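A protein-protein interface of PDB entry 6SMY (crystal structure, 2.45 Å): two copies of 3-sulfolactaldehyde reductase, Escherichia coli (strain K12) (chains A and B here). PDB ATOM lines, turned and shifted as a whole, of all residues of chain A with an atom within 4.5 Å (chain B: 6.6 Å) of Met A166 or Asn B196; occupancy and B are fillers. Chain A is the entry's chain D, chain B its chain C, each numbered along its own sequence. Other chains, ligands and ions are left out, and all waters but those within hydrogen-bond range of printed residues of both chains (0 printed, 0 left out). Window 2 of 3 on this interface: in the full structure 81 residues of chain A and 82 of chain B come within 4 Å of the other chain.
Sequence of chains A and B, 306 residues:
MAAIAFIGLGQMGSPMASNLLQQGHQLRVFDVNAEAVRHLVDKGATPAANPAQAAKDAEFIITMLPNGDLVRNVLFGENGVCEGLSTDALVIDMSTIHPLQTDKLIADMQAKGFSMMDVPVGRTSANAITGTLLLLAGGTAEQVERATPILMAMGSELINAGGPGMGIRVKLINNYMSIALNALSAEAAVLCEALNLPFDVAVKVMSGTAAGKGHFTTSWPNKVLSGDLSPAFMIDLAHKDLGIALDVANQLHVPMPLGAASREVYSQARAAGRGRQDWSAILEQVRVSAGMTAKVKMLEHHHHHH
O of Ala A161 touches CG1 of Val B201, at 3.9 Å.
Leu B197 touches Met A166.
Leu B197 touches Arg A169.
Val A170 touches Leu B197 (CA to CD2, 3.6 Å).
No position is printed for both chains.
Of the 6 pairs that touch across the chains among the printed residues, none has its exchanged pair printed and touching as well.
The backbone carbonyl oxygen of Cys B192 sits at hydrogen-bond distance from the backbone NH of Leu B197, at 3.2 Å.
The side-chain carboxylate (OD2) of Asp A118 sits at hydrogen-bond distance from the backbone NH (N) of Met A166.
The guanidinium group (NH1) of Arg A169 sits at hydrogen-bond distance from the backbone carbonyl oxygen (O) of Gly A165, 3.0 Å away.
Printed residues of chain B that touch a printed residue of chain A: Leu B195, Asn B196, Leu B197 and Val B201.
Hydrophobic or aromatic side chains of chain B within 4 Å of the printed part of chain A: Leu B195, Leu B197 and Val B201.
Among the printed residues, 6 pairs touch across the chains.
Among the printed residues, no Asp or Glu carboxylate lies within 4 Å of a Lys or Arg side-chain nitrogen of the other chain.
Of the printed residues of chain B, Ala A161 touches Val B201 (3.9 Å).
Gly A165 touches none of the printed residues of chain B.
Of the printed residues of chain B, Arg A169 touches Leu B195 (2.5 Å) and Leu B197 (3.9 Å).
Of the printed residues of chain B, Val A170 touches Leu B197 (3.6 Å).
Of the printed residues of chain A, Leu B195 touches Arg A169 (2.5 Å).
Asn B196 touches just one residue of chain A: Met A166.
Of the printed residues of chain A, Val B201 touches Ala A161 (3.9 Å).
The nearest residue of chain B that does not touch Met A166 is Leu B195 (4.4 Å).
NE of Arg A169 is in hydrogen-bond range of O of Leu B195 (2.5 Å).
The side-chain sulfur (SD) of Met A166 sits close to the backbone carbonyl oxygen (O) of Asn B196.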
ATOM      1  N   ASP A 118     -34.392 -17.569  -5.913  1.00  0.00           N
ATOM      2  CA  ASP A 118     -34.023 -16.135  -5.925  1.00  0.00           C
ATOM      3  C   ASP A 118     -34.601 -15.505  -7.197  1.00  0.00           C
ATOM      4  O   ASP A 118     -34.161 -15.887  -8.298  1.00  0.00           O
ATOM      5  CB  ASP A 118     -32.500 -15.973  -5.874  1.00  0.00           C
ATOM      6  CG  ASP A 118     -31.779 -16.768  -6.947  1.00  0.00           C
ATOM      7  OD1 ASP A 118     -32.073 -17.998  -7.045  1.00  0.00           O
ATOM      8  OD2 ASP A 118     -30.946 -16.173  -7.683  1.00  0.00           O
ATOM      9  N   ALA A 161     -32.096 -16.773 -15.480  1.00  0.00           N
ATOM     10  CA  ALA A 161     -30.684 -16.594 -15.063  1.00  0.00           C
ATOM     11  C   ALA A 161     -29.937 -17.934 -15.152  1.00  0.00           C
ATOM     12  O   ALA A 161     -28.683 -17.925 -15.210  1.00  0.00           O
ATOM     13  CB  ALA A 161     -30.676 -16.023 -13.671  1.00  0.00           C
ATOM     14  N   GLY A 162     -30.675 -19.051 -15.134  1.00  0.00           N
ATOM     15  CA  GLY A 162     -30.166 -20.390 -15.489  1.00  0.00           C
ATOM     16  C   GLY A 162     -29.596 -21.151 -14.305  1.00  0.00           C
ATOM     17  O   GLY A 162     -28.598 -21.840 -14.486  1.00  0.00           O
ATOM     18  N   GLY A 163     -30.184 -21.014 -13.124  1.00  0.00           N
ATOM     19  CA  GLY A 163     -29.893 -21.889 -11.975  1.00  0.00           C
ATOM     20  C   GLY A 163     -30.188 -21.208 -10.640  1.00  0.00           C
ATOM     21  O   GLY A 163     -30.374 -19.995 -10.588  1.00  0.00           O
ATOM     22  N   PRO A 164     -30.239 -21.973  -9.519  1.00  0.00           N
ATOM     23  CA  PRO A 164     -30.301 -21.381  -8.183  1.00  0.00           C
ATOM     24  C   PRO A 164     -29.151 -20.389  -7.965  1.00  0.00           C
ATOM     25  O   PRO A 164     -28.039 -20.727  -8.279  1.00  0.00           O
ATOM     26  CB  PRO A 164     -30.181 -22.595  -7.239  1.00  0.00           C
ATOM     27  CG  PRO A 164     -30.688 -23.752  -8.071  1.00  0.00           C
ATOM     28  CD  PRO A 164     -30.207 -23.443  -9.474  1.00  0.00           C
ATOM     29  N   GLY A 165     -29.478 -19.191  -7.469  1.00  0.00           N
ATOM     30  CA  GLY A 165     -28.512 -18.133  -7.082  1.00  0.00           C
ATOM     31  C   GLY A 165     -28.060 -17.291  -8.266  1.00  0.00           C
ATOM     32  O   GLY A 165     -27.323 -16.308  -8.033  1.00  0.00           O
ATOM     33  N   MET A 166     -28.469 -17.645  -9.486  1.00  0.00           N
ATOM     34  CA  MET A 166     -28.028 -16.939 -10.709  1.00  0.00           C
ATOM     35  C   MET A 166     -28.848 -15.660 -10.866  1.00  0.00           C
ATOM     36  O   MET A 166     -28.398 -14.787 -11.575  1.00  0.00           O
ATOM     37  CB  MET A 166     -28.183 -17.825 -11.954  1.00  0.00           C
ATOM     38  CG  MET A 166     -27.280 -19.060 -11.933  1.00  0.00           C
ATOM     39  SD  MET A 166     -25.524 -18.690 -11.752  1.00  0.00           S
ATOM     40  CE  MET A 166     -25.100 -19.764 -10.379  1.00  0.00           C
ATOM     41  N   GLY A 167     -30.006 -15.587 -10.220  1.00  0.00           N
ATOM     42  CA  GLY A 167     -30.893 -14.417 -10.239  1.00  0.00           C
ATOM     43  C   GLY A 167     -30.244 -13.243  -9.523  1.00  0.00           C
ATOM     44  O   GLY A 167     -30.051 -12.155 -10.149  1.00  0.00           O
ATOM     45  N   ILE A 168     -29.852 -13.477  -8.271  1.00  0.00           N
ATOM     46  CA  ILE A 168     -29.158 -12.465  -7.432  1.00  0.00           C
ATOM     47  C   ILE A 168     -27.811 -12.082  -8.080  1.00  0.00           C
ATOM     48  O   ILE A 168     -27.478 -10.864  -8.088  1.00  0.00           O
ATOM     49  CB  ILE A 168     -29.033 -12.960  -5.976  1.00  0.00           C
ATOM     50  CG1 ILE A 168     -28.516 -11.850  -5.066  1.00  0.00           C
ATOM     51  CG2 ILE A 168     -28.195 -14.226  -5.873  1.00  0.00           C
ATOM     52  CD1 ILE A 168     -29.322 -10.561  -5.181  1.00  0.00           C
ATOM     53  N   ARG A 169     -27.110 -13.070  -8.662  1.00  0.00           N
ATOM     54  CA  ARG A 169     -25.772 -12.870  -9.259  1.00  0.00           C
ATOM     55  C   ARG A 169     -25.896 -11.885 -10.418  1.00  0.00           C
ATOM     56  O   ARG A 169     -25.151 -10.919 -10.410  1.00  0.00           O
ATOM     57  CB  ARG A 169     -25.158 -14.200  -9.699  1.00  0.00           C
ATOM     58  CG  ARG A 169     -24.517 -14.992  -8.571  1.00  0.00           C
ATOM     59  CD  ARG A 169     -24.196 -16.424  -8.961  1.00  0.00           C
ATOM     60  NE  ARG A 169     -23.403 -17.137  -7.967  1.00  0.00           N
ATOM     61  CZ  ARG A 169     -23.841 -17.513  -6.756  1.00  0.00           C
ATOM     62  NH1 ARG A 169     -25.068 -17.227  -6.347  1.00  0.00           N
ATOM     63  NH2 ARG A 169     -23.029 -18.150  -5.939  1.00  0.00           N
ATOM     64  N   VAL A 170     -26.835 -12.107 -11.350  1.00  0.00           N
ATOM     65  CA  VAL A 170     -26.946 -11.275 -12.575  1.00  0.00           C
ATOM     66  C   VAL A 170     -27.451  -9.893 -12.167  1.00  0.00           C
ATOM     67  O   VAL A 170     -27.007  -8.901 -12.813  1.00  0.00           O
ATOM     68  CB  VAL A 170     -27.825 -11.929 -13.659  1.00  0.00           C
ATOM     69  CG1 VAL A 170     -29.318 -11.888 -13.322  1.00  0.00           C
ATOM     70  CG2 VAL A 170     -27.547 -11.302 -15.018  1.00  0.00           C
ATOM     71  N   LEU B 191     -15.809 -10.646 -11.639  1.00  0.00           N
ATOM     72  CA  LEU B 191     -16.754 -10.883 -10.511  1.00  0.00           C
ATOM     73  C   LEU B 191     -17.829 -11.874 -10.989  1.00  0.00           C
ATOM     74  O   LEU B 191     -18.171 -12.800 -10.228  1.00  0.00           O
ATOM     75  CB  LEU B 191     -17.367  -9.566 -10.037  1.00  0.00           C
ATOM     76  CG  LEU B 191     -18.272  -9.670  -8.804  1.00  0.00           C
ATOM     77  CD1 LEU B 191     -17.507 -10.139  -7.581  1.00  0.00           C
ATOM     78  CD2 LEU B 191     -18.932  -8.350  -8.483  1.00  0.00           C
ATOM     79  N   CYS B 192     -18.313 -11.684 -12.213  1.00  0.00           N
ATOM     80  CA  CYS B 192     -19.223 -12.612 -12.924  1.00  0.00           C
ATOM     81  C   CYS B 192     -18.658 -14.040 -12.876  1.00  0.00           C
ATOM     82  O   CYS B 192     -19.361 -14.922 -12.388  1.00  0.00           O
ATOM     83  CB  CYS B 192     -19.442 -12.168 -14.367  1.00  0.00           C
ATOM     84  SG  CYS B 192     -20.951 -12.899 -15.023  1.00  0.00           S
ATOM     85  N   GLU B 193     -17.422 -14.235 -13.341  1.00  0.00           N
ATOM     86  CA  GLU B 193     -16.731 -15.550 -13.363  1.00  0.00           C
ATOM     87  C   GLU B 193     -16.573 -16.088 -11.933  1.00  0.00           C
ATOM     88  O   GLU B 193     -16.872 -17.284 -11.733  1.00  0.00           O
ATOM     89  CB  GLU B 193     -15.392 -15.455 -14.093  1.00  0.00           C
ATOM     90  CG  GLU B 193     -14.600 -16.753 -14.155  1.00  0.00           C
ATOM     91  CD  GLU B 193     -13.355 -16.680 -15.038  1.00  0.00           C
ATOM     92  OE1 GLU B 193     -13.203 -15.698 -15.766  1.00  0.00           O
ATOM     93  OE2 GLU B 193     -12.515 -17.606 -14.999  1.00  0.00           O
ATOM     94  N   ALA B 194     -16.180 -15.257 -10.962  1.00  0.00           N
ATOM     95  CA  ALA B 194     -15.953 -15.688  -9.557  1.00  0.00           C
ATOM     96  C   ALA B 194     -17.262 -16.192  -8.946  1.00  0.00           C
ATOM     97  O   ALA B 194     -17.212 -17.100  -8.104  1.00  0.00           O
ATOM     98  CB  ALA B 194     -15.372 -14.578  -8.724  1.00  0.00           C
ATOM     99  N   LEU B 195     -18.393 -15.621  -9.371  1.00  0.00           N
ATOM    100  CA  LEU B 195     -19.742 -16.019  -8.903  1.00  0.00           C
ATOM    101  C   LEU B 195     -20.308 -17.193  -9.717  1.00  0.00           C
ATOM    102  O   LEU B 195     -21.416 -17.595  -9.401  1.00  0.00           O
ATOM    103  CB  LEU B 195     -20.653 -14.795  -8.994  1.00  0.00           C
ATOM    104  CG  LEU B 195     -20.494 -13.799  -7.852  1.00  0.00           C
ATOM    105  CD1 LEU B 195     -21.254 -12.516  -8.144  1.00  0.00           C
ATOM    106  CD2 LEU B 195     -20.959 -14.427  -6.547  1.00  0.00           C
ATOM    107  N   ASN B 196     -19.565 -17.718 -10.701  1.00  0.00           N
ATOM    108  CA  ASN B 196     -19.939 -18.879 -11.557  1.00  0.00           C
ATOM    109  C   ASN B 196     -21.228 -18.574 -12.323  1.00  0.00           C
ATOM    110  O   ASN B 196     -22.056 -19.480 -12.453  1.00  0.00           O
ATOM    111  CB  ASN B 196     -20.058 -20.170 -10.740  1.00  0.00           C
ATOM    112  CG  ASN B 196     -18.772 -20.502 -10.008  1.00  0.00           C
ATOM    113  OD1 ASN B 196     -18.724 -20.524  -8.782  1.00  0.00           O
ATOM    114  ND2 ASN B 196     -17.706 -20.720 -10.749  1.00  0.00           N
ATOM    115  N   LEU B 197     -21.379 -17.340 -12.808  1.00  0.00           N
ATOM    116  CA  LEU B 197     -22.499 -16.900 -13.678  1.00  0.00           C
ATOM    117  C   LEU B 197     -21.954 -16.837 -15.098  1.00  0.00           C
ATOM    118  O   LEU B 197     -20.925 -16.214 -15.331  1.00  0.00           O
ATOM    119  CB  LEU B 197     -22.995 -15.542 -13.179  1.00  0.00           C
ATOM    120  CG  LEU B 197     -24.084 -14.869 -14.020  1.00  0.00           C
ATOM    121  CD1 LEU B 197     -25.409 -15.612 -13.951  1.00  0.00           C
ATOM    122  CD2 LEU B 197     -24.280 -13.439 -13.588  1.00  0.00           C
ATOM    123  N   PRO B 198     -22.543 -17.538 -16.089  1.00  0.00           N
ATOM    124  CA  PRO B 198     -22.088 -17.396 -17.472  1.00  0.00           C
ATOM    125  C   PRO B 198     -22.131 -15.919 -17.876  1.00  0.00           C
ATOM    126  O   PRO B 198     -23.091 -15.234 -17.580  1.00  0.00           O
ATOM    127  CB  PRO B 198     -23.068 -18.227 -18.300  1.00  0.00           C
ATOM    128  CG  PRO B 198     -23.657 -19.215 -17.283  1.00  0.00           C
ATOM    129  CD  PRO B 198     -23.651 -18.489 -15.952  1.00  0.00           C
ATOM    130  N   VAL B 201     -24.997 -14.499 -20.112  1.00  0.00           N
ATOM    131  CA  VAL B 201     -26.242 -14.167 -19.357  1.00  0.00           C
ATOM    132  C   VAL B 201     -26.148 -12.728 -18.815  1.00  0.00           C
ATOM    133  O   VAL B 201     -27.133 -11.934 -18.956  1.00  0.00           O
ATOM    134  CB  VAL B 201     -26.488 -15.202 -18.242  1.00  0.00           C
ATOM    135  CG1 VAL B 201     -27.646 -14.824 -17.320  1.00  0.00           C
ATOM    136  CG2 VAL B 201     -26.720 -16.587 -18.836  1.00  0.00           C
